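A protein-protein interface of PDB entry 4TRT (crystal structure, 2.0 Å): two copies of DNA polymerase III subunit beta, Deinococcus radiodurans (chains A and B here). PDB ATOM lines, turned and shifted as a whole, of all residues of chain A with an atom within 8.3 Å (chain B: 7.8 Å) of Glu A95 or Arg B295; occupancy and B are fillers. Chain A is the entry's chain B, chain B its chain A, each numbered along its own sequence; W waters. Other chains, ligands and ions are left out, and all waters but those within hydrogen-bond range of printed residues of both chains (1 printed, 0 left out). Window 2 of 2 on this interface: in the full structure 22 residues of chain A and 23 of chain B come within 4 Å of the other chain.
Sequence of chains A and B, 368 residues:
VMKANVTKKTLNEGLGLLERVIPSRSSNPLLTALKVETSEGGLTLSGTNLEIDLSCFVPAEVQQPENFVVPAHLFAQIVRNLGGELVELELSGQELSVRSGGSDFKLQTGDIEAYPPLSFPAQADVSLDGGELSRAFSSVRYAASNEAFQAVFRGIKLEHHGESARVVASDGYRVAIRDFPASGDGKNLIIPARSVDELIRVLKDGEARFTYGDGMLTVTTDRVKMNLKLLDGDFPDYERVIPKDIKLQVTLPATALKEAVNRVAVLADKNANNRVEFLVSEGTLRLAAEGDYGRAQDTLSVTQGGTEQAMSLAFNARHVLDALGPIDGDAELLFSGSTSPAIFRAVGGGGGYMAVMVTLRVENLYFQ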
ATOM      1  N   VAL A   1     -21.575  14.769 -23.067  1.00  0.00           N
ATOM      2  CA  VAL A   1     -21.058  15.739 -22.057  1.00  0.00           C
ATOM      3  C   VAL A   1     -21.555  17.152 -22.334  1.00  0.00           C
ATOM      4  O   VAL A   1     -21.913  17.486 -23.464  1.00  0.00           O
ATOM      5  CB  VAL A   1     -19.514  15.771 -22.044  1.00  0.00           C
ATOM      6  CG1 VAL A   1     -18.941  14.378 -21.747  1.00  0.00           C
ATOM      7  CG2 VAL A   1     -18.978  16.296 -23.376  1.00  0.00           C
ATOM      8  N   MET A   2     -21.553  17.986 -21.303  1.00  0.00           N
ATOM      9  CA  MET A   2     -21.909  19.391 -21.472  1.00  0.00           C
ATOM     10  C   MET A   2     -20.889  20.155 -22.296  1.00  0.00           C
ATOM     11  O   MET A   2     -19.680  20.034 -22.085  1.00  0.00           O
ATOM     12  CB  MET A   2     -22.075  20.102 -20.136  1.00  0.00           C
ATOM     13  CG  MET A   2     -22.735  21.464 -20.283  1.00  0.00           C
ATOM     14  SD  MET A   2     -21.558  22.834 -20.277  1.00  0.00           S
ATOM     15  CE  MET A   2     -21.066  22.765 -18.555  1.00  0.00           C
ATOM     16  N   PHE A  68     -21.709  23.524 -12.398  1.00  0.00           N
ATOM     17  CA  PHE A  68     -20.407  23.271 -11.802  1.00  0.00           C
ATOM     18  C   PHE A  68     -19.891  24.504 -11.091  1.00  0.00           C
ATOM     19  O   PHE A  68     -20.410  25.608 -11.285  1.00  0.00           O
ATOM     20  CB  PHE A  68     -19.387  22.834 -12.883  1.00  0.00           C
ATOM     21  CG  PHE A  68     -19.162  23.854 -13.965  1.00  0.00           C
ATOM     22  CD1 PHE A  68     -19.963  23.879 -15.098  1.00  0.00           C
ATOM     23  CD2 PHE A  68     -18.132  24.770 -13.868  1.00  0.00           C
ATOM     24  CE1 PHE A  68     -19.753  24.814 -16.106  1.00  0.00           C
ATOM     25  CE2 PHE A  68     -17.916  25.706 -14.860  1.00  0.00           C
ATOM     26  CZ  PHE A  68     -18.730  25.731 -15.988  1.00  0.00           C
ATOM     27  N   VAL A  69     -18.875  24.308 -10.254  1.00  0.00           N
ATOM     28  CA  VAL A  69     -18.156  25.421  -9.639  1.00  0.00           C
ATOM     29  C   VAL A  69     -16.682  25.364 -10.013  1.00  0.00           C
ATOM     30  O   VAL A  69     -16.119  24.279 -10.171  1.00  0.00           O
ATOM     31  CB  VAL A  69     -18.321  25.475  -8.095  1.00  0.00           C
ATOM     32  CG1 VAL A  69     -19.788  25.712  -7.707  1.00  0.00           C
ATOM     33  CG2 VAL A  69     -17.770  24.226  -7.440  1.00  0.00           C
ATOM     34  N   VAL A  70     -16.079  26.541 -10.196  1.00  0.00           N
ATOM     35  CA  VAL A  70     -14.650  26.672 -10.490  1.00  0.00           C
ATOM     36  C   VAL A  70     -14.114  27.888  -9.737  1.00  0.00           C
ATOM     37  O   VAL A  70     -14.886  28.782  -9.416  1.00  0.00           O
ATOM     38  CB  VAL A  70     -14.399  26.861 -12.007  1.00  0.00           C
ATOM     39  CG1 VAL A  70     -14.621  25.547 -12.753  1.00  0.00           C
ATOM     40  CG2 VAL A  70     -15.285  27.975 -12.570  1.00  0.00           C
ATOM     41  N   LEU A  74      -9.255  32.693 -11.112  1.00  0.00           N
ATOM     42  CA  LEU A  74      -8.475  31.899 -12.051  1.00  0.00           C
ATOM     43  C   LEU A  74      -9.208  31.725 -13.381  1.00  0.00           C
ATOM     44  O   LEU A  74      -8.620  31.916 -14.451  1.00  0.00           O
ATOM     45  CB  LEU A  74      -8.112  30.537 -11.452  1.00  0.00           C
ATOM     46  CG  LEU A  74      -7.329  29.578 -12.350  1.00  0.00           C
ATOM     47  CD1 LEU A  74      -6.037  30.219 -12.841  1.00  0.00           C
ATOM     48  CD2 LEU A  74      -7.040  28.296 -11.577  1.00  0.00           C
ATOM     49  N   ILE A  78      -7.968  33.141 -17.056  1.00  0.00           N
ATOM     50  CA  ILE A  78      -7.796  32.246 -18.220  1.00  0.00           C
ATOM     51  C   ILE A  78      -8.602  32.765 -19.415  1.00  0.00           C
ATOM     52  O   ILE A  78      -8.096  32.832 -20.539  1.00  0.00           O
ATOM     53  CB  ILE A  78      -8.209  30.794 -17.847  1.00  0.00           C
ATOM     54  CG1 ILE A  78      -7.141  30.165 -16.941  1.00  0.00           C
ATOM     55  CG2 ILE A  78      -8.475  29.922 -19.072  1.00  0.00           C
ATOM     56  CD1 ILE A  78      -7.560  28.840 -16.327  1.00  0.00           C
ATOM     57  N   LEU A  89     -16.541  25.754 -23.976  1.00  0.00           N
ATOM     58  CA  LEU A  89     -16.485  25.127 -22.664  1.00  0.00           C
ATOM     59  C   LEU A  89     -16.962  23.694 -22.828  1.00  0.00           C
ATOM     60  O   LEU A  89     -17.897  23.423 -23.605  1.00  0.00           O
ATOM     61  CB  LEU A  89     -17.386  25.863 -21.658  1.00  0.00           C
ATOM     62  CG  LEU A  89     -17.052  27.330 -21.388  1.00  0.00           C
ATOM     63  CD1 LEU A  89     -18.066  27.983 -20.436  1.00  0.00           C
ATOM     64  CD2 LEU A  89     -15.624  27.455 -20.852  1.00  0.00           C
ATOM     65  N   GLU A  90     -16.305  22.785 -22.118  1.00  0.00           N
ATOM     66  CA  GLU A  90     -16.727  21.394 -22.058  1.00  0.00           C
ATOM     67  C   GLU A  90     -16.504  20.879 -20.643  1.00  0.00           C
ATOM     68  O   GLU A  90     -15.471  21.129 -20.046  1.00  0.00           O
ATOM     69  CB  GLU A  90     -15.975  20.526 -23.084  1.00  0.00           C
ATOM     70  CG  GLU A  90     -16.340  19.044 -23.027  1.00  0.00           C
ATOM     71  CD  GLU A  90     -15.525  18.176 -23.984  1.00  0.00           C
ATOM     72  OE1 GLU A  90     -14.994  18.686 -24.996  1.00  0.00           O
ATOM     73  OE2 GLU A  90     -15.428  16.963 -23.718  1.00  0.00           O
ATOM     74  N   LEU A  91     -17.480  20.157 -20.110  1.00  0.00           N
ATOM     75  CA  LEU A  91     -17.370  19.610 -18.766  1.00  0.00           C
ATOM     76  C   LEU A  91     -17.407  18.093 -18.843  1.00  0.00           C
ATOM     77  O   LEU A  91     -18.402  17.525 -19.279  1.00  0.00           O
ATOM     78  CB  LEU A  91     -18.504  20.131 -17.874  1.00  0.00           C
ATOM     79  CG  LEU A  91     -18.439  19.672 -16.412  1.00  0.00           C
ATOM     80  CD1 LEU A  91     -17.279  20.344 -15.692  1.00  0.00           C
ATOM     81  CD2 LEU A  91     -19.761  19.938 -15.710  1.00  0.00           C
ATOM     82  N   SER A  92     -16.321  17.452 -18.425  1.00  0.00           N
ATOM     83  CA  SER A  92     -16.249  15.986 -18.363  1.00  0.00           C
ATOM     84  C   SER A  92     -15.693  15.594 -17.007  1.00  0.00           C
ATOM     85  O   SER A  92     -14.560  15.946 -16.682  1.00  0.00           O
ATOM     86  CB  SER A  92     -15.383  15.391 -19.477  1.00  0.00           C
ATOM     87  OG  SER A  92     -15.864  15.799 -20.743  1.00  0.00           O
ATOM     88  N   GLY A  93     -16.493  14.874 -16.224  1.00  0.00           N
ATOM     89  CA  GLY A  93     -16.135  14.523 -14.855  1.00  0.00           C
ATOM     90  C   GLY A  93     -15.942  15.779 -14.023  1.00  0.00           C
ATOM     91  O   GLY A  93     -16.805  16.656 -14.021  1.00  0.00           O
ATOM     92  N   GLN A  94     -14.798  15.876 -13.348  1.00  0.00           N
ATOM     93  CA  GLN A  94     -14.461  17.053 -12.549  1.00  0.00           C
ATOM     94  C   GLN A  94     -13.517  18.018 -13.289  1.00  0.00           C
ATOM     95  O   GLN A  94     -12.746  18.737 -12.662  1.00  0.00           O
ATOM     96  CB  GLN A  94     -13.831  16.628 -11.221  1.00  0.00           C
ATOM     97  CG  GLN A  94     -14.823  16.085 -10.234  1.00  0.00           C
ATOM     98  CD  GLN A  94     -14.174  15.308  -9.103  1.00  0.00           C
ATOM     99  OE1 GLN A  94     -13.166  15.735  -8.532  1.00  0.00           O
ATOM    100  NE2 GLN A  94     -14.752  14.156  -8.770  1.00  0.00           N
ATOM    101  N   GLU A  95     -13.585  18.037 -14.616  1.00  0.00           N
ATOM    102  CA  GLU A  95     -12.654  18.817 -15.414  1.00  0.00           C
ATOM    103  C   GLU A  95     -13.414  19.703 -16.387  1.00  0.00           C
ATOM    104  O   GLU A  95     -14.196  19.205 -17.205  1.00  0.00           O
ATOM    105  CB  GLU A  95     -11.726  17.874 -16.175  1.00  0.00           C
ATOM    106  CG  GLU A  95     -10.480  18.542 -16.723  1.00  0.00           C
ATOM    107  CD  GLU A  95      -9.478  17.542 -17.281  1.00  0.00           C
ATOM    108  OE1 GLU A  95      -9.648  17.097 -18.434  1.00  0.00           O
ATOM    109  OE2 GLU A  95      -8.521  17.201 -16.563  1.00  0.00           O
ATOM    110  N   LEU A  96     -13.218  21.017 -16.272  1.00  0.00           N
ATOM    111  CA  LEU A  96     -13.735  21.950 -17.262  1.00  0.00           C
ATOM    112  C   LEU A  96     -12.659  22.249 -18.312  1.00  0.00           C
ATOM    113  O   LEU A  96     -11.582  22.744 -17.987  1.00  0.00           O
ATOM    114  CB  LEU A  96     -14.168  23.256 -16.606  1.00  0.00           C
ATOM    115  CG  LEU A  96     -14.723  24.303 -17.578  1.00  0.00           C
ATOM    116  CD1 LEU A  96     -16.121  23.931 -18.091  1.00  0.00           C
ATOM    117  CD2 LEU A  96     -14.725  25.658 -16.874  1.00  0.00           C
ATOM    118  N   SER A  97     -12.971  21.970 -19.570  1.00  0.00           N
ATOM    119  CA  SER A  97     -12.088  22.335 -20.675  1.00  0.00           C
ATOM    120  C   SER A  97     -12.492  23.701 -21.220  1.00  0.00           C
ATOM    121  O   SER A  97     -13.678  23.979 -21.395  1.00  0.00           O
ATOM    122  CB  SER A  97     -12.136  21.273 -21.772  1.00  0.00           C
ATOM    123  OG  SER A  97     -11.601  20.066 -21.291  1.00  0.00           O
ATOM    124  N   VAL A  98     -11.499  24.566 -21.426  1.00  0.00           N
ATOM    125  CA  VAL A  98     -11.724  25.930 -21.920  1.00  0.00           C
ATOM    126  C   VAL A  98     -10.808  26.089 -23.130  1.00  0.00           C
ATOM    127  O   VAL A  98      -9.579  26.027 -22.997  1.00  0.00           O
ATOM    128  CB  VAL A  98     -11.374  27.023 -20.866  1.00  0.00           C
ATOM    129  CG1 VAL A  98     -11.699  28.427 -21.391  1.00  0.00           C
ATOM    130  CG2 VAL A  98     -12.058  26.755 -19.529  1.00  0.00           C
ATOM    131  N   ARG A  99     -11.417  26.274 -24.296  1.00  0.00           N
ATOM    132  CA  ARG A  99     -10.718  26.197 -25.559  1.00  0.00           C
ATOM    133  C   ARG A  99     -11.007  27.416 -26.412  1.00  0.00           C
ATOM    134  O   ARG A  99     -12.146  27.855 -26.503  1.00  0.00           O
ATOM    135  CB  ARG A  99     -11.149  24.950 -26.353  1.00  0.00           C
ATOM    136  CG  ARG A  99     -10.761  23.628 -25.732  1.00  0.00           C
ATOM    137  CD  ARG A  99     -11.036  22.470 -26.667  1.00  0.00           C
ATOM    138  NE  ARG A  99     -10.758  21.202 -25.991  1.00  0.00           N
ATOM    139  CZ  ARG A  99     -11.670  20.393 -25.440  1.00  0.00           C
ATOM    140  NH1 ARG A  99     -12.970  20.675 -25.478  1.00  0.00           N
ATOM    141  NH2 ARG A  99     -11.271  19.269 -24.853  1.00  0.00           N
ATOM    142  N   ASP A 104      -5.913  25.260 -25.118  1.00  0.00           N
ATOM    143  CA  ASP A 104      -6.735  24.227 -24.461  1.00  0.00           C
ATOM    144  C   ASP A 104      -6.362  24.211 -22.981  1.00  0.00           C
ATOM    145  O   ASP A 104      -5.280  23.758 -22.621  1.00  0.00           O
ATOM    146  CB  ASP A 104      -6.459  22.862 -25.100  1.00  0.00           C
ATOM    147  CG  ASP A 104      -7.410  21.759 -24.621  1.00  0.00           C
ATOM    148  OD1 ASP A 104      -8.246  21.980 -23.721  1.00  0.00           O
ATOM    149  OD2 ASP A 104      -7.307  20.640 -25.151  1.00  0.00           O
ATOM    150  N   PHE A 105      -7.253  24.718 -22.136  1.00  0.00           N
ATOM    151  CA  PHE A 105      -7.024  24.817 -20.700  1.00  0.00           C
ATOM    152  C   PHE A 105      -7.962  23.815 -20.008  1.00  0.00           C
ATOM    153  O   PHE A 105      -9.110  23.659 -20.435  1.00  0.00           O
ATOM    154  CB  PHE A 105      -7.290  26.266 -20.217  1.00  0.00           C
ATOM    155  CG  PHE A 105      -6.183  27.227 -20.542  1.00  0.00           C
ATOM    156  CD1 PHE A 105      -5.949  27.623 -21.850  1.00  0.00           C
ATOM    157  CD2 PHE A 105      -5.335  27.700 -19.549  1.00  0.00           C
ATOM    158  CE1 PHE A 105      -4.891  28.467 -22.164  1.00  0.00           C
ATOM    159  CE2 PHE A 105      -4.285  28.551 -19.855  1.00  0.00           C
ATOM    160  CZ  PHE A 105      -4.061  28.932 -21.167  1.00  0.00           C
ATOM    161  N   LYS A 106      -7.476  23.134 -18.968  1.00  0.00           N
ATOM    162  CA  LYS A 106      -8.316  22.265 -18.129  1.00  0.00           C
ATOM    163  C   LYS A 106      -8.302  22.788 -16.700  1.00  0.00           C
ATOM    164  O   LYS A 106      -7.233  22.931 -16.124  1.00  0.00           O
ATOM    165  CB  LYS A 106      -7.802  20.827 -18.091  1.00  0.00           C
ATOM    166  CG  LYS A 106      -7.406  20.208 -19.414  1.00  0.00           C
ATOM    167  CD  LYS A 106      -8.573  20.044 -20.368  1.00  0.00           C
ATOM    168  CE  LYS A 106      -8.166  19.132 -21.517  1.00  0.00           C
ATOM    169  NZ  LYS A 106      -9.080  19.320 -22.675  1.00  0.00           N
ATOM    170  N   LEU A 107      -9.478  23.073 -16.136  1.00  0.00           N
ATOM    171  CA  LEU A 107      -9.602  23.469 -14.717  1.00  0.00           C
ATOM    172  C   LEU A 107     -10.308  22.385 -13.928  1.00  0.00           C
ATOM    173  O   LEU A 107     -11.348  21.883 -14.362  1.00  0.00           O
ATOM    174  CB  LEU A 107     -10.426  24.752 -14.560  1.00  0.00           C
ATOM    175  CG  LEU A 107      -9.796  26.085 -14.924  1.00  0.00           C
ATOM    176  CD1 LEU A 107     -10.715  27.214 -14.478  1.00  0.00           C
ATOM    177  CD2 LEU A 107      -8.406  26.224 -14.306  1.00  0.00           C
ATOM    178  N   GLN A 108      -9.759  22.045 -12.766  1.00  0.00           N
ATOM    179  CA  GLN A 108     -10.466  21.174 -11.829  1.00  0.00           C
ATOM    180  C   GLN A 108     -11.685  21.934 -11.280  1.00  0.00           C
ATOM    181  O   GLN A 108     -11.584  23.086 -10.854  1.00  0.00           O
ATOM    182  CB  GLN A 108      -9.557  20.695 -10.680  1.00  0.00           C
ATOM    183  CG  GLN A 108      -8.817  19.381 -10.927  1.00  0.00           C
ATOM    184  CD  GLN A 108      -9.743  18.176 -10.940  1.00  0.00           C
ATOM    185  OE1 GLN A 108      -9.673  17.352 -11.840  1.00  0.00           O
ATOM    186  NE2 GLN A 108     -10.618  18.074  -9.940  1.00  0.00           N
ATOM    187  N   THR A 109     -12.844  21.296 -11.347  1.00  0.00           N
ATOM    188  CA  THR A 109     -14.067  21.864 -10.790  1.00  0.00           C
ATOM    189  C   THR A 109     -14.142  21.488  -9.305  1.00  0.00           C
ATOM    190  O   THR A 109     -13.466  20.555  -8.860  1.00  0.00           O
ATOM    191  CB  THR A 109     -15.311  21.312 -11.503  1.00  0.00           C
ATOM    192  OG1 THR A 109     -15.297  19.890 -11.410  1.00  0.00           O
ATOM    193  CG2 THR A 109     -15.345  21.720 -12.977  1.00  0.00           C
ATOM    194  N   GLY A 110     -14.993  22.188  -8.556  1.00  0.00           N
ATOM    195  CA  GLY A 110     -15.107  21.982  -7.120  1.00  0.00           C
ATOM    196  C   GLY A 110     -16.364  21.234  -6.712  1.00  0.00           C
ATOM    197  O   GLY A 110     -17.059  20.645  -7.540  1.00  0.00           O
ATOM    198  N   VAL B 264      -0.304  30.228 -20.806  1.00  0.00           N
ATOM    199  CA  VAL B 264      -0.064  28.875 -20.296  1.00  0.00           C
ATOM    200  C   VAL B 264       0.565  28.890 -18.899  1.00  0.00           C
ATOM    201  O   VAL B 264       0.242  28.059 -18.063  1.00  0.00           O
ATOM    202  CB  VAL B 264       0.787  28.062 -21.299  1.00  0.00           C
ATOM    203  CG1 VAL B 264       1.271  26.758 -20.682  1.00  0.00           C
ATOM    204  CG2 VAL B 264      -0.044  27.777 -22.538  1.00  0.00           C
ATOM    205  N   LEU B 267      -1.115  28.378 -15.243  1.00  0.00           N
ATOM    206  CA  LEU B 267      -1.374  27.077 -14.592  1.00  0.00           C
ATOM    207  C   LEU B 267      -0.122  26.315 -14.100  1.00  0.00           C
ATOM    208  O   LEU B 267      -0.249  25.224 -13.546  1.00  0.00           O
ATOM    209  CB  LEU B 267      -2.236  26.176 -15.486  1.00  0.00           C
ATOM    210  CG  LEU B 267      -3.707  26.618 -15.560  1.00  0.00           C
ATOM    211  CD1 LEU B 267      -4.506  25.658 -16.419  1.00  0.00           C
ATOM    212  CD2 LEU B 267      -4.372  26.753 -14.181  1.00  0.00           C
ATOM    213  N   ALA B 268       1.064  26.911 -14.249  1.00  0.00           N
ATOM    214  CA  ALA B 268       2.297  26.360 -13.661  1.00  0.00           C
ATOM    215  C   ALA B 268       2.232  26.501 -12.135  1.00  0.00           C
ATOM    216  O   ALA B 268       1.577  27.417 -11.620  1.00  0.00           O
ATOM    217  CB  ALA B 268       3.526  27.066 -14.237  1.00  0.00           C
ATOM    218  N   ALA B 288       3.180  23.747 -22.665  1.00  0.00           N
ATOM    219  CA  ALA B 288       2.365  23.045 -21.660  1.00  0.00           C
ATOM    220  C   ALA B 288       2.815  23.405 -20.258  1.00  0.00           C
ATOM    221  O   ALA B 288       4.013  23.577 -19.994  1.00  0.00           O
ATOM    222  CB  ALA B 288       2.428  21.535 -21.850  1.00  0.00           C
ATOM    223  N   ALA B 289       1.846  23.529 -19.360  1.00  0.00           N
ATOM    224  CA  ALA B 289       2.121  23.681 -17.948  1.00  0.00           C
ATOM    225  C   ALA B 289       1.008  23.019 -17.171  1.00  0.00           C
ATOM    226  O   ALA B 289      -0.111  22.835 -17.677  1.00  0.00           O
ATOM    227  CB  ALA B 289       2.255  25.156 -17.570  1.00  0.00           C
ATOM    228  N   GLU B 290       1.319  22.653 -15.939  1.00  0.00           N
ATOM    229  CA  GLU B 290       0.395  21.894 -15.119  1.00  0.00           C
ATOM    230  C   GLU B 290       0.702  22.153 -13.663  1.00  0.00           C
ATOM    231  O   GLU B 290       1.858  22.323 -13.292  1.00  0.00           O
ATOM    232  CB  GLU B 290       0.528  20.406 -15.430  1.00  0.00           C
ATOM    233  CG  GLU B 290      -0.459  19.533 -14.691  1.00  0.00           C
ATOM    234  CD  GLU B 290      -0.497  18.108 -15.219  1.00  0.00           C
ATOM    235  OE1 GLU B 290       0.250  17.799 -16.173  1.00  0.00           O
ATOM    236  OE2 GLU B 290      -1.272  17.293 -14.669  1.00  0.00           O
ATOM    237  N   GLY B 291      -0.349  22.203 -12.856  1.00  0.00           N
ATOM    238  CA  GLY B 291      -0.231  22.462 -11.430  1.00  0.00           C
ATOM    239  C   GLY B 291      -1.447  21.968 -10.686  1.00  0.00           C
ATOM    240  O   GLY B 291      -2.219  21.162 -11.206  1.00  0.00           O
ATOM    241  N   ASP B 292      -1.623  22.470  -9.466  1.00  0.00           N
ATOM    242  CA  ASP B 292      -2.695  22.015  -8.594  1.00  0.00           C
ATOM    243  C   ASP B 292      -4.096  22.367  -9.094  1.00  0.00           C
ATOM    244  O   ASP B 292      -5.057  21.675  -8.756  1.00  0.00           O
ATOM    245  CB  ASP B 292      -2.510  22.589  -7.186  1.00  0.00           C
ATOM    246  CG  ASP B 292      -1.301  22.007  -6.468  1.00  0.00           C
ATOM    247  OD1 ASP B 292      -1.017  20.801  -6.638  1.00  0.00           O
ATOM    248  OD2 ASP B 292      -0.644  22.757  -5.717  1.00  0.00           O
ATOM    249  N   TYR B 293      -4.212  23.425  -9.897  1.00  0.00           N
ATOM    250  CA  TYR B 293      -5.528  23.917 -10.348  1.00  0.00           C
ATOM    251  C   TYR B 293      -5.987  23.312 -11.668  1.00  0.00           C
ATOM    252  O   TYR B 293      -7.182  23.294 -11.973  1.00  0.00           O
ATOM    253  CB  TYR B 293      -5.515  25.435 -10.467  1.00  0.00           C
ATOM    254  CG  TYR B 293      -5.309  26.119  -9.141  1.00  0.00           C
ATOM    255  CD1 TYR B 293      -6.378  26.314  -8.268  1.00  0.00           C
ATOM    256  CD2 TYR B 293      -4.046  26.551  -8.749  1.00  0.00           C
ATOM    257  CE1 TYR B 293      -6.196  26.934  -7.043  1.00  0.00           C
ATOM    258  CE2 TYR B 293      -3.857  27.172  -7.524  1.00  0.00           C
ATOM    259  CZ  TYR B 293      -4.932  27.360  -6.677  1.00  0.00           C
ATOM    260  OH  TYR B 293      -4.749  27.974  -5.462  1.00  0.00           O
ATOM    261  N   GLY B 294      -5.033  22.819 -12.444  1.00  0.00           N
ATOM    262  CA  GLY B 294      -5.328  22.218 -13.727  1.00  0.00           C
ATOM    263  C   GLY B 294      -4.096  22.218 -14.607  1.00  0.00           C
ATOM    264  O   GLY B 294      -2.969  22.241 -14.107  1.00  0.00           O
ATOM    265  N   ARG B 295      -4.320  22.206 -15.918  1.00  0.00           N
ATOM    266  CA  ARG B 295      -3.245  22.084 -16.912  1.00  0.00           C
ATOM    267  C   ARG B 295      -3.625  22.856 -18.166  1.00  0.00           C
ATOM    268  O   ARG B 295      -4.820  22.991 -18.471  1.00  0.00           O
ATOM    269  CB  ARG B 295      -2.982  20.600 -17.211  1.00  0.00           C
ATOM    270  CG  ARG B 295      -3.929  19.967 -18.219  1.00  0.00           C
ATOM    271  CD  ARG B 295      -4.203  18.481 -17.971  1.00  0.00           C
ATOM    272  NE  ARG B 295      -4.720  17.824 -19.186  1.00  0.00           N
ATOM    273  CZ  ARG B 295      -5.615  16.832 -19.199  1.00  0.00           C
ATOM    274  NH1 ARG B 295      -6.148  16.360 -18.070  1.00  0.00           N
ATOM    275  NH2 ARG B 295      -6.001  16.318 -20.366  1.00  0.00           N
ATOM    276  N   ALA B 296      -2.619  23.384 -18.865  1.00  0.00           N
ATOM    277  CA  ALA B 296      -2.825  24.231 -20.038  1.00  0.00           C
ATOM    278  C   ALA B 296      -1.914  23.780 -21.143  1.00  0.00           C
ATOM    279  O   ALA B 296      -0.755  23.470 -20.873  1.00  0.00           O
ATOM    280  CB  ALA B 296      -2.491  25.683 -19.712  1.00  0.00           C
ATOM    281  N   GLN B 297      -2.415  23.821 -22.375  1.00  0.00           N
ATOM    282  CA  GLN B 297      -1.586  23.658 -23.565  1.00  0.00           C
ATOM    283  C   GLN B 297      -1.986  24.679 -24.621  1.00  0.00           C
ATOM    284  O   GLN B 297      -3.180  24.941 -24.811  1.00  0.00           O
ATOM    285  CB  GLN B 297      -1.777  22.274 -24.174  1.00  0.00           C
ATOM    286  CG  GLN B 297      -1.243  21.135 -23.316  1.00  0.00           C
ATOM    287  CD  GLN B 297      -1.438  19.764 -23.941  1.00  0.00           C
ATOM    288  OE1 GLN B 297      -2.224  19.602 -24.876  1.00  0.00           O
ATOM    289  NE2 GLN B 297      -0.730  18.765 -23.413  1.00  0.00           N
HETATM  290  O   HOH W   1      -9.269  24.636 -10.596  1.00  0.00           O
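Water W1 lies within hydrogen-bond range of O of Gln A108 and O of Tyr B293.
Leu A74 touches Tyr B293 (CD2 to CB, 3.4 Å).
Ala B296 touches Asp A104.
Val B264 touches Phe A105.
Leu B267 touches Phe A105 (CD1 to CD2, 3.8 Å).
Phe A105 touches Arg B295.
Ala B296 touches Phe A105 (CB to CE2, 3.4 Å).
Lys A106 touches Leu B267 (O to CD1, 3.9 Å).
CA of Gly B294 touches O of Lys A106, at 3.1 Å.
Leu A107 touches Tyr B293.
Of the printed residues of chain B, Leu A74 touches Tyr B293 (3.4 Å).
Glu A95 touches one residue of chain B.
Of the printed residues of chain A, Leu B267 touches Phe A105 and Lys A106.
Glu B290 touches none of the printed residues of chain A.
Gly B291 touches none of the printed residues of chain A.
Of the printed residues of chain A, Gly B294 touches Lys A106 (3.1 Å).
Arg B295 touches three residues of chain A.
Ala B296 touches just these residues of chain A: Asp A104 (3.6 Å) and Phe A105 (3.4 Å).
The nearest residue of chain B that does not touch Glu A95 is Gly B294 (6.6 Å).
The nearest residue of chain A that does not touch Arg B295 is Asp A104 (4.2 Å).
The nearest printed residue of chain B that does not touch Asp A104 is Arg B295 (4.2 Å).
The backbone NH (N) of Gln A108 is in hydrogen-bond range of the backbone carbonyl oxygen (O) of Tyr B293 (3.0 Å).
The guanidinium group of Arg B295 is in salt-bridge range of the side-chain carboxylate of Glu A95, at 2.9 Å.
N of Lys A106 sits at hydrogen-bond distance from O of Arg B295, at 2.7 Å.
The backbone NH (N) of Asp A104 lies within hydrogen-bond range of the backbone carbonyl oxygen (O) of Gln B297, at 2.8 Å.
O of Leu B267 sits at hydrogen-bond distance from N of Gly B291 (3.1 Å).
The backbone carbonyl oxygen (O) of Ala B289 is in hydrogen-bond range of the backbone NH (N) of Ala B296.
O of Gln A94 lies close to OE1 of Gln A108.
The backbone carbonyl oxygen (O) of Leu A107 is in hydrogen-bond range of the backbone NH (N) of Leu A96, at 2.8 Å.
O of Phe A105 lies within hydrogen-bond range of N of Val A98 (2.7 Å).
The side-chain amino group (NZ) of Lys A106 lies within salt-bridge range of the side-chain carboxylate (OD1) of Asp A104, 3.0 Å away.
No position is printed for both chains.
Of the 13 pairs that touch across the chains among the printed residues, none has its exchanged pair printed and touching as well.
Hydrophobic or aromatic side chains of chain B that line the printed part of chain A: Leu B267, Tyr B293 and Ala B296.
Of the 25 printed residues of chain A, 7 touch a printed residue of chain B.
Hydrophobic or aromatic side chains of chain A that line the printed part of chain B: Leu A74, Phe A105 and Leu A107.
Among the printed residues, Asp or Glu carboxylates within 4 Å of a Lys or Arg side-chain nitrogen of the other chain: Glu A95 with Arg B295 (2.9 Å).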
